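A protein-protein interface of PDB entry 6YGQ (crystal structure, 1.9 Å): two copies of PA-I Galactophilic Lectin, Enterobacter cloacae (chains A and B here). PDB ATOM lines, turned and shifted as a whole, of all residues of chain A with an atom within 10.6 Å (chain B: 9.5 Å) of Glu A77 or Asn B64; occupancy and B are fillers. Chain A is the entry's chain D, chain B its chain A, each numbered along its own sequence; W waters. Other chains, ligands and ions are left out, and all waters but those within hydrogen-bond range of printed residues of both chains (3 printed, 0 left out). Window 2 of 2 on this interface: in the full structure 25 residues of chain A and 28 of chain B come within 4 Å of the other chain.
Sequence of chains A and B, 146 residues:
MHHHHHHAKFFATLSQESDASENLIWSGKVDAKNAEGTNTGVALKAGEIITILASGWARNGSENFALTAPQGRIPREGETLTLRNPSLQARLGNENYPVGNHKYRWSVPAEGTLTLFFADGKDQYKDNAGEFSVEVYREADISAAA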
ATOM      1  N   ARG A  59     -18.197  17.222  22.981  1.00  0.00           N
ATOM      2  CA  ARG A  59     -19.080  17.132  24.135  1.00  0.00           C
ATOM      3  C   ARG A  59     -18.559  16.069  25.094  1.00  0.00           C
ATOM      4  O   ARG A  59     -18.122  14.996  24.669  1.00  0.00           O
ATOM      5  CB  ARG A  59     -20.509  16.792  23.705  1.00  0.00           C
ATOM      6  CG  ARG A  59     -21.296  17.978  23.167  1.00  0.00           C
ATOM      7  CD  ARG A  59     -22.797  17.819  23.399  1.00  0.00           C
ATOM      8  NE  ARG A  59     -23.426  19.091  23.752  1.00  0.00           N
ATOM      9  CZ  ARG A  59     -23.843  19.995  22.869  1.00  0.00           C
ATOM     10  NH1 ARG A  59     -23.709  19.772  21.568  1.00  0.00           N
ATOM     11  NH2 ARG A  59     -24.399  21.124  23.289  1.00  0.00           N
ATOM     12  N   ASN A  64     -26.810  20.192  26.985  1.00  0.00           N
ATOM     13  CA  ASN A  64     -26.373  21.441  26.372  1.00  0.00           C
ATOM     14  C   ASN A  64     -25.128  21.978  27.063  1.00  0.00           C
ATOM     15  O   ASN A  64     -24.203  22.473  26.409  1.00  0.00           O
ATOM     16  CB  ASN A  64     -27.504  22.469  26.445  1.00  0.00           C
ATOM     17  CG  ASN A  64     -28.037  22.648  27.860  1.00  0.00           C
ATOM     18  OD1 ASN A  64     -28.086  21.696  28.642  1.00  0.00           O
ATOM     19  ND2 ASN A  64     -28.433  23.871  28.197  1.00  0.00           N
ATOM     20  N   PHE A  65     -25.095  21.884  28.395  1.00  0.00           N
ATOM     21  CA  PHE A  65     -23.956  22.357  29.173  1.00  0.00           C
ATOM     22  C   PHE A  65     -22.640  21.777  28.665  1.00  0.00           C
ATOM     23  O   PHE A  65     -21.609  22.463  28.654  1.00  0.00           O
ATOM     24  CB  PHE A  65     -24.147  21.957  30.641  1.00  0.00           C
ATOM     25  CG  PHE A  65     -24.770  23.017  31.511  1.00  0.00           C
ATOM     26  CD1 PHE A  65     -24.646  22.936  32.889  1.00  0.00           C
ATOM     27  CD2 PHE A  65     -25.483  24.075  30.971  1.00  0.00           C
ATOM     28  CE1 PHE A  65     -25.207  23.894  33.711  1.00  0.00           C
ATOM     29  CE2 PHE A  65     -26.048  25.039  31.791  1.00  0.00           C
ATOM     30  CZ  PHE A  65     -25.910  24.946  33.162  1.00  0.00           C
ATOM     31  N   ALA A  66     -22.658  20.514  28.242  1.00  0.00           N
ATOM     32  CA  ALA A  66     -21.459  19.677  28.232  1.00  0.00           C
ATOM     33  C   ALA A  66     -20.702  19.820  26.913  1.00  0.00           C
ATOM     34  O   ALA A  66     -20.590  18.891  26.112  1.00  0.00           O
ATOM     35  CB  ALA A  66     -21.839  18.225  28.503  1.00  0.00           C
ATOM     36  N   LEU A  67     -20.152  21.016  26.711  1.00  0.00           N
ATOM     37  CA  LEU A  67     -19.362  21.337  25.530  1.00  0.00           C
ATOM     38  C   LEU A  67     -17.945  21.701  25.949  1.00  0.00           C
ATOM     39  O   LEU A  67     -17.738  22.334  26.990  1.00  0.00           O
ATOM     40  CB  LEU A  67     -19.972  22.501  24.746  1.00  0.00           C
ATOM     41  CG  LEU A  67     -20.807  22.158  23.513  1.00  0.00           C
ATOM     42  CD1 LEU A  67     -21.481  23.421  22.994  1.00  0.00           C
ATOM     43  CD2 LEU A  67     -19.964  21.508  22.427  1.00  0.00           C
ATOM     44  N   ARG A  73     -13.690  23.017  29.152  1.00  0.00           N
ATOM     45  CA  ARG A  73     -15.136  23.145  29.062  1.00  0.00           C
ATOM     46  C   ARG A  73     -15.560  24.609  28.991  1.00  0.00           C
ATOM     47  O   ARG A  73     -14.845  25.521  29.415  1.00  0.00           O
ATOM     48  CB  ARG A  73     -15.819  22.465  30.253  1.00  0.00           C
ATOM     49  CG  ARG A  73     -15.836  23.257  31.566  1.00  0.00           C
ATOM     50  CD  ARG A  73     -16.729  22.547  32.581  1.00  0.00           C
ATOM     51  NE  ARG A  73     -16.619  23.059  33.945  1.00  0.00           N
ATOM     52  CZ  ARG A  73     -17.222  24.159  34.389  1.00  0.00           C
ATOM     53  NH1 ARG A  73     -17.976  24.887  33.573  1.00  0.00           N
ATOM     54  NH2 ARG A  73     -17.069  24.535  35.652  1.00  0.00           N
ATOM     55  N   ILE A  74     -16.756  24.821  28.453  1.00  0.00           N
ATOM     56  CA  ILE A  74     -17.325  26.161  28.359  1.00  0.00           C
ATOM     57  C   ILE A  74     -17.745  26.602  29.755  1.00  0.00           C
ATOM     58  O   ILE A  74     -18.083  25.755  30.597  1.00  0.00           O
ATOM     59  CB  ILE A  74     -18.511  26.207  27.383  1.00  0.00           C
ATOM     60  CG1 ILE A  74     -19.617  25.242  27.813  1.00  0.00           C
ATOM     61  CG2 ILE A  74     -18.050  25.887  25.966  1.00  0.00           C
ATOM     62  CD1 ILE A  74     -20.960  25.554  27.170  1.00  0.00           C
ATOM     63  N   PRO A  75     -17.718  27.899  30.055  1.00  0.00           N
ATOM     64  CA  PRO A  75     -18.363  28.373  31.283  1.00  0.00           C
ATOM     65  C   PRO A  75     -19.865  28.151  31.216  1.00  0.00           C
ATOM     66  O   PRO A  75     -20.480  28.235  30.149  1.00  0.00           O
ATOM     67  CB  PRO A  75     -18.020  29.869  31.322  1.00  0.00           C
ATOM     68  CG  PRO A  75     -16.855  30.030  30.410  1.00  0.00           C
ATOM     69  CD  PRO A  75     -17.006  28.978  29.348  1.00  0.00           C
ATOM     70  N   ARG A  76     -20.452  27.869  32.373  1.00  0.00           N
ATOM     71  CA  ARG A  76     -21.886  27.694  32.499  1.00  0.00           C
ATOM     72  C   ARG A  76     -22.509  28.969  33.059  1.00  0.00           C
ATOM     73  O   ARG A  76     -21.819  29.927  33.418  1.00  0.00           O
ATOM     74  CB  ARG A  76     -22.197  26.483  33.377  1.00  0.00           C
ATOM     75  CG  ARG A  76     -22.009  25.160  32.653  1.00  0.00           C
ATOM     76  CD  ARG A  76     -21.439  24.077  33.556  1.00  0.00           C
ATOM     77  NE  ARG A  76     -21.129  22.861  32.806  1.00  0.00           N
ATOM     78  CZ  ARG A  76     -20.493  21.807  33.309  1.00  0.00           C
ATOM     79  NH1 ARG A  76     -20.093  21.810  34.575  1.00  0.00           N
ATOM     80  NH2 ARG A  76     -20.257  20.748  32.547  1.00  0.00           N
ATOM     81  N   GLU A  77     -23.839  28.977  33.135  1.00  0.00           N
ATOM     82  CA  GLU A  77     -24.556  30.154  33.603  1.00  0.00           C
ATOM     83  C   GLU A  77     -24.056  30.572  34.979  1.00  0.00           C
ATOM     84  O   GLU A  77     -23.925  29.745  35.887  1.00  0.00           O
ATOM     85  CB  GLU A  77     -26.057  29.877  33.653  1.00  0.00           C
ATOM     86  CG  GLU A  77     -26.906  31.133  33.783  1.00  0.00           C
ATOM     87  CD  GLU A  77     -28.376  30.827  33.989  1.00  0.00           C
ATOM     88  OE1 GLU A  77     -28.914  29.969  33.259  1.00  0.00           O
ATOM     89  OE2 GLU A  77     -28.994  31.444  34.882  1.00  0.00           O
ATOM     90  N   GLY A  78     -23.775  31.864  35.129  1.00  0.00           N
ATOM     91  CA  GLY A  78     -23.326  32.411  36.386  1.00  0.00           C
ATOM     92  C   GLY A  78     -21.854  32.240  36.677  1.00  0.00           C
ATOM     93  O   GLY A  78     -21.380  32.759  37.696  1.00  0.00           O
ATOM     94  N   GLU A  79     -21.116  31.537  35.828  1.00  0.00           N
ATOM     95  CA  GLU A  79     -19.696  31.328  36.048  1.00  0.00           C
ATOM     96  C   GLU A  79     -18.877  32.407  35.352  1.00  0.00           C
ATOM     97  O   GLU A  79     -19.299  32.985  34.346  1.00  0.00           O
ATOM     98  CB  GLU A  79     -19.262  29.955  35.532  1.00  0.00           C
ATOM     99  CG  GLU A  79     -19.767  28.782  36.351  1.00  0.00           C
ATOM    100  CD  GLU A  79     -19.181  27.462  35.886  1.00  0.00           C
ATOM    101  OE1 GLU A  79     -18.914  27.323  34.674  1.00  0.00           O
ATOM    102  OE2 GLU A  79     -18.985  26.566  36.732  1.00  0.00           O
ATOM    103  N   THR A  80     -17.694  32.670  35.898  1.00  0.00           N
ATOM    104  CA  THR A  80     -16.745  33.538  35.222  1.00  0.00           C
ATOM    105  C   THR A  80     -16.276  32.879  33.927  1.00  0.00           C
ATOM    106  O   THR A  80     -16.432  31.673  33.719  1.00  0.00           O
ATOM    107  CB  THR A  80     -15.544  33.834  36.117  1.00  0.00           C
ATOM    108  OG1 THR A  80     -14.828  32.620  36.376  1.00  0.00           O
ATOM    109  CG2 THR A  80     -15.993  34.457  37.435  1.00  0.00           C
ATOM    110  N   LEU A  81     -15.687  33.688  33.049  1.00  0.00           N
ATOM    111  CA  LEU A  81     -15.237  33.221  31.745  1.00  0.00           C
ATOM    112  C   LEU A  81     -13.819  32.649  31.778  1.00  0.00           C
ATOM    113  O   LEU A  81     -13.151  32.605  30.739  1.00  0.00           O
ATOM    114  CB  LEU A  81     -15.329  34.360  30.727  1.00  0.00           C
ATOM    115  CG  LEU A  81     -16.735  34.943  30.565  1.00  0.00           C
ATOM    116  CD1 LEU A  81     -16.761  36.070  29.542  1.00  0.00           C
ATOM    117  CD2 LEU A  81     -17.728  33.852  30.178  1.00  0.00           C
ATOM    118  N   ARG A  84     -10.751  26.724  32.195  1.00  0.00           N
ATOM    119  CA  ARG A  84     -10.763  25.654  33.177  1.00  0.00           C
ATOM    120  C   ARG A  84      -9.885  24.511  32.662  1.00  0.00           C
ATOM    121  O   ARG A  84      -9.027  24.720  31.791  1.00  0.00           O
ATOM    122  CB  ARG A  84     -12.222  25.288  33.466  1.00  0.00           C
ATOM    123  CG  ARG A  84     -12.929  26.461  34.167  1.00  0.00           C
ATOM    124  CD  ARG A  84     -14.396  26.235  34.493  1.00  0.00           C
ATOM    125  NE  ARG A  84     -14.856  27.220  35.475  1.00  0.00           N
ATOM    126  CZ  ARG A  84     -15.291  28.442  35.174  1.00  0.00           C
ATOM    127  NH1 ARG A  84     -15.347  28.848  33.912  1.00  0.00           N
ATOM    128  NH2 ARG A  84     -15.678  29.261  36.143  1.00  0.00           N
ATOM    129  N   TRP B  57     -12.370  32.641  26.674  1.00  0.00           N
ATOM    130  CA  TRP B  57     -13.811  32.598  26.467  1.00  0.00           C
ATOM    131  C   TRP B  57     -14.358  34.017  26.402  1.00  0.00           C
ATOM    132  O   TRP B  57     -14.076  34.838  27.282  1.00  0.00           O
ATOM    133  CB  TRP B  57     -14.520  31.836  27.590  1.00  0.00           C
ATOM    134  CG  TRP B  57     -14.174  30.379  27.677  1.00  0.00           C
ATOM    135  CD1 TRP B  57     -13.506  29.760  28.693  1.00  0.00           C
ATOM    136  CD2 TRP B  57     -14.491  29.357  26.724  1.00  0.00           C
ATOM    137  NE1 TRP B  57     -13.383  28.416  28.432  1.00  0.00           N
ATOM    138  CE2 TRP B  57     -13.979  28.143  27.228  1.00  0.00           C
ATOM    139  CE3 TRP B  57     -15.156  29.349  25.493  1.00  0.00           C
ATOM    140  CZ2 TRP B  57     -14.110  26.935  26.543  1.00  0.00           C
ATOM    141  CZ3 TRP B  57     -15.282  28.152  24.816  1.00  0.00           C
ATOM    142  CH2 TRP B  57     -14.762  26.961  25.341  1.00  0.00           C
ATOM    143  N   ALA B  58     -15.152  34.295  25.374  1.00  0.00           N
ATOM    144  CA  ALA B  58     -15.810  35.584  25.229  1.00  0.00           C
ATOM    145  C   ALA B  58     -17.250  35.356  24.803  1.00  0.00           C
ATOM    146  O   ALA B  58     -17.539  34.447  24.021  1.00  0.00           O
ATOM    147  CB  ALA B  58     -15.092  36.470  24.205  1.00  0.00           C
ATOM    148  N   ARG B  59     -18.152  36.181  25.324  1.00  0.00           N
ATOM    149  CA  ARG B  59     -19.556  36.146  24.936  1.00  0.00           C
ATOM    150  C   ARG B  59     -19.823  37.253  23.925  1.00  0.00           C
ATOM    151  O   ARG B  59     -19.374  38.389  24.110  1.00  0.00           O
ATOM    152  CB  ARG B  59     -20.463  36.311  26.155  1.00  0.00           C
ATOM    153  CG  ARG B  59     -20.380  35.167  27.152  1.00  0.00           C
ATOM    154  CD  ARG B  59     -20.678  35.651  28.564  1.00  0.00           C
ATOM    155  NE  ARG B  59     -22.099  35.928  28.759  1.00  0.00           N
ATOM    156  CZ  ARG B  59     -22.580  36.859  29.579  1.00  0.00           C
ATOM    157  NH1 ARG B  59     -21.758  37.620  30.292  1.00  0.00           N
ATOM    158  NH2 ARG B  59     -23.890  37.030  29.685  1.00  0.00           N
ATOM    159  N   ASN B  60     -20.544  36.919  22.854  1.00  0.00           N
ATOM    160  CA  ASN B  60     -20.986  37.913  21.886  1.00  0.00           C
ATOM    161  C   ASN B  60     -22.414  38.374  22.151  1.00  0.00           C
ATOM    162  O   ASN B  60     -23.006  39.054  21.308  1.00  0.00           O
ATOM    163  CB  ASN B  60     -20.853  37.373  20.456  1.00  0.00           C
ATOM    164  CG  ASN B  60     -21.626  36.087  20.228  1.00  0.00           C
ATOM    165  OD1 ASN B  60     -22.430  35.668  21.059  1.00  0.00           O
ATOM    166  ND2 ASN B  60     -21.385  35.453  19.084  1.00  0.00           N
ATOM    167  N   GLY B  61     -22.969  38.029  23.308  1.00  0.00           N
ATOM    168  CA  GLY B  61     -24.307  38.446  23.679  1.00  0.00           C
ATOM    169  C   GLY B  61     -24.575  38.057  25.116  1.00  0.00           C
ATOM    170  O   GLY B  61     -23.733  37.457  25.788  1.00  0.00           O
ATOM    171  N   SER B  62     -25.775  38.404  25.583  1.00  0.00           N
ATOM    172  CA  SER B  62     -26.156  38.129  26.962  1.00  0.00           C
ATOM    173  C   SER B  62     -26.730  36.732  27.161  1.00  0.00           C
ATOM    174  O   SER B  62     -26.765  36.251  28.300  1.00  0.00           O
ATOM    175  CB  SER B  62     -27.182  39.161  27.446  1.00  0.00           C
ATOM    176  OG  SER B  62     -26.635  40.468  27.451  1.00  0.00           O
ATOM    177  N   GLU B  63     -27.174  36.072  26.094  1.00  0.00           N
ATOM    178  CA  GLU B  63     -27.790  34.759  26.229  1.00  0.00           C
ATOM    179  C   GLU B  63     -26.748  33.700  26.578  1.00  0.00           C
ATOM    180  O   GLU B  63     -25.562  33.833  26.268  1.00  0.00           O
ATOM    181  CB  GLU B  63     -28.511  34.373  24.937  1.00  0.00           C
ATOM    182  CG  GLU B  63     -29.515  35.407  24.453  1.00  0.00           C
ATOM    183  CD  GLU B  63     -28.921  36.363  23.435  1.00  0.00           C
ATOM    184  OE1 GLU B  63     -29.635  36.741  22.482  1.00  0.00           O
ATOM    185  OE2 GLU B  63     -27.737  36.732  23.587  1.00  0.00           O
ATOM    186  N   ASN B  64     -27.211  32.629  27.228  1.00  0.00           N
ATOM    187  CA  ASN B  64     -26.294  31.575  27.649  1.00  0.00           C
ATOM    188  C   ASN B  64     -25.585  30.936  26.462  1.00  0.00           C
ATOM    189  O   ASN B  64     -24.423  30.529  26.579  1.00  0.00           O
ATOM    190  CB  ASN B  64     -27.046  30.514  28.454  1.00  0.00           C
ATOM    191  CG  ASN B  64     -27.290  30.936  29.892  1.00  0.00           C
ATOM    192  OD1 ASN B  64     -26.638  31.847  30.403  1.00  0.00           O
ATOM    193  ND2 ASN B  64     -28.234  30.274  30.552  1.00  0.00           N
ATOM    194  N   PHE B  65     -26.254  30.844  25.314  1.00  0.00           N
ATOM    195  CA  PHE B  65     -25.652  30.250  24.128  1.00  0.00           C
ATOM    196  C   PHE B  65     -24.706  31.198  23.401  1.00  0.00           C
ATOM    197  O   PHE B  65     -24.073  30.784  22.423  1.00  0.00           O
ATOM    198  CB  PHE B  65     -26.746  29.777  23.159  1.00  0.00           C
ATOM    199  CG  PHE B  65     -27.578  30.891  22.579  1.00  0.00           C
ATOM    200  CD1 PHE B  65     -28.818  31.200  23.114  1.00  0.00           C
ATOM    201  CD2 PHE B  65     -27.125  31.620  21.490  1.00  0.00           C
ATOM    202  CE1 PHE B  65     -29.586  32.221  22.580  1.00  0.00           C
ATOM    203  CE2 PHE B  65     -27.886  32.642  20.955  1.00  0.00           C
ATOM    204  CZ  PHE B  65     -29.118  32.942  21.499  1.00  0.00           C
ATOM    205  N   ALA B  66     -24.584  32.444  23.850  1.00  0.00           N
ATOM    206  CA  ALA B  66     -23.812  33.454  23.127  1.00  0.00           C
ATOM    207  C   ALA B  66     -22.346  33.436  23.566  1.00  0.00           C
ATOM    208  O   ALA B  66     -21.790  34.435  24.016  1.00  0.00           O
ATOM    209  CB  ALA B  66     -24.435  34.831  23.335  1.00  0.00           C
ATOM    210  N   LEU B  67     -21.720  32.270  23.407  1.00  0.00           N
ATOM    211  CA  LEU B  67     -20.345  32.040  23.827  1.00  0.00           C
ATOM    212  C   LEU B  67     -19.447  31.770  22.627  1.00  0.00           C
ATOM    213  O   LEU B  67     -19.879  31.184  21.630  1.00  0.00           O
ATOM    214  CB  LEU B  67     -20.259  30.849  24.784  1.00  0.00           C
ATOM    215  CG  LEU B  67     -20.126  31.127  26.279  1.00  0.00           C
ATOM    216  CD1 LEU B  67     -20.279  29.816  27.033  1.00  0.00           C
ATOM    217  CD2 LEU B  67     -18.802  31.795  26.605  1.00  0.00           C
ATOM    218  N   THR B  68     -18.182  32.182  22.742  1.00  0.00           N
ATOM    219  CA  THR B  68     -17.198  31.962  21.692  1.00  0.00           C
ATOM    220  C   THR B  68     -15.833  31.658  22.301  1.00  0.00           C
ATOM    221  O   THR B  68     -15.533  32.070  23.423  1.00  0.00           O
ATOM    222  CB  THR B  68     -17.040  33.183  20.765  1.00  0.00           C
ATOM    223  OG1 THR B  68     -16.264  34.194  21.428  1.00  0.00           O
ATOM    224  CG2 THR B  68     -18.386  33.755  20.372  1.00  0.00           C
ATOM    225  N   ILE B  74     -19.816  28.732  19.730  1.00  0.00           N
ATOM    226  CA  ILE B  74     -20.097  27.348  20.097  1.00  0.00           C
ATOM    227  C   ILE B  74     -21.227  26.822  19.221  1.00  0.00           C
ATOM    228  O   ILE B  74     -22.099  27.595  18.798  1.00  0.00           O
ATOM    229  CB  ILE B  74     -20.457  27.213  21.587  1.00  0.00           C
ATOM    230  CG1 ILE B  74     -21.732  27.993  21.921  1.00  0.00           C
ATOM    231  CG2 ILE B  74     -19.302  27.681  22.459  1.00  0.00           C
ATOM    232  CD1 ILE B  74     -22.346  27.600  23.258  1.00  0.00           C
ATOM    233  N   PRO B  75     -21.249  25.524  18.921  1.00  0.00           N
ATOM    234  CA  PRO B  75     -22.437  24.943  18.286  1.00  0.00           C
ATOM    235  C   PRO B  75     -23.670  25.183  19.140  1.00  0.00           C
ATOM    236  O   PRO B  75     -23.605  25.184  20.372  1.00  0.00           O
ATOM    237  CB  PRO B  75     -22.096  23.451  18.186  1.00  0.00           C
ATOM    238  CG  PRO B  75     -20.605  23.399  18.193  1.00  0.00           C
ATOM    239  CD  PRO B  75     -20.148  24.552  19.048  1.00  0.00           C
ATOM    240  N   ARG B  76     -24.799  25.395  18.474  1.00  0.00           N
ATOM    241  CA  ARG B  76     -26.050  25.685  19.149  1.00  0.00           C
ATOM    242  C   ARG B  76     -26.953  24.454  19.128  1.00  0.00           C
ATOM    243  O   ARG B  76     -26.596  23.390  18.614  1.00  0.00           O
ATOM    244  CB  ARG B  76     -26.746  26.884  18.500  1.00  0.00           C
ATOM    245  CG  ARG B  76     -26.312  28.244  19.047  1.00  0.00           C
ATOM    246  CD  ARG B  76     -26.126  29.238  17.911  1.00  0.00           C
ATOM    247  NE  ARG B  76     -25.968  30.620  18.357  1.00  0.00           N
ATOM    248  CZ  ARG B  76     -24.900  31.093  18.995  1.00  0.00           C
ATOM    249  NH1 ARG B  76     -23.881  30.295  19.292  1.00  0.00           N
ATOM    250  NH2 ARG B  76     -24.858  32.372  19.345  1.00  0.00           N
HETATM  251  O   HOH W   1     -11.256  33.284  29.371  1.00  0.00           O
HETATM  252  O   HOH W   2     -12.059  26.136  29.672  1.00  0.00           O
HETATM  253  O   HOH W   3     -14.636  27.562  31.448  1.00  0.00           O
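The side-chain carboxylate (OE1) of Glu A77 sits at hydrogen-bond distance from the side-chain amide nitrogen (ND2) of Asn B64, at 2.8 Å. NE1 of Trp B57 lies close to O of Arg A73 (3.4 Å).
NH2 of Arg B59 is in hydrogen-bond range of O of Ser B62, at 3.3 Å. The backbone NH of Ile A74 lies within hydrogen-bond range of the backbone carbonyl oxygen of Leu A67, at 3.0 Å. The backbone NH (N) of Ile B74 sits at hydrogen-bond distance from the backbone carbonyl oxygen (O) of Leu B67 (3.1 Å). NH1 of Arg A73 lies within salt-bridge range of OE1 of Glu A79, 2.8 Å away.
Among the printed residues, pairs that only touch across the chains: Pro A75 with Leu B67, Ile A74 with Trp B57, Leu A81 with Trp B57, Pro A75 with Trp B57, Leu A67 with Pro B75 and Leu A81 with Arg B59.
Of the printed residues of chain B, Pro A75 touches Trp B57 and Leu B67. Arg A76 touches none of the printed residues of chain B. Thr A80 touches none of the printed residues of chain B. Printed residues of chain B within 4 Å of Leu A81: Trp B57 and Arg B59. No residue of chain A comes within 4 Å of Phe B65. No residue of chain A comes within 4 Å of Ala B66. Printed residues of chain A within 4 Å of Leu B67: Pro A75. The nearest residue of chain B that does not touch Glu A77 is Leu B67 (7.1 Å). The nearest printed residue of chain A that does not touch Leu B67 is Ile A74 (4.03 Å).
Printed residues of chain B that touch a printed residue of chain A: Trp B57, Arg B59, Asn B64, Leu B67 and Pro B75. Of the 15 printed residues of chain A, 6 touch a printed residue of chain B. Hydrophobic or aromatic side chains of chain A that line the printed part of chain B: Leu A67, Ile A74, Pro A75 and Leu A81. Among the printed residues, 8 pairs touch across the chains.
Leu A67 touches Pro B75, and with the chains exchanged Pro A75 touches Leu B67.
Water W1 bridges the backbone carbonyl oxygen (O) of Leu A81 (2.4 Å) and the backbone NH (N) of Trp B57 (3.0 Å). Water W2 lies within hydrogen-bond range of the backbone carbonyl oxygen of Arg A73, the backbone NH of Arg A84 and the indole nitrogen of Trp B57. Water W3 lies within hydrogen-bond range of the guanidinium group of Arg A84 (2.9 Å), the backbone carbonyl oxygen of Arg A73 (2.9 Å) and the indole nitrogen of Trp B57 (3.4 Å).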
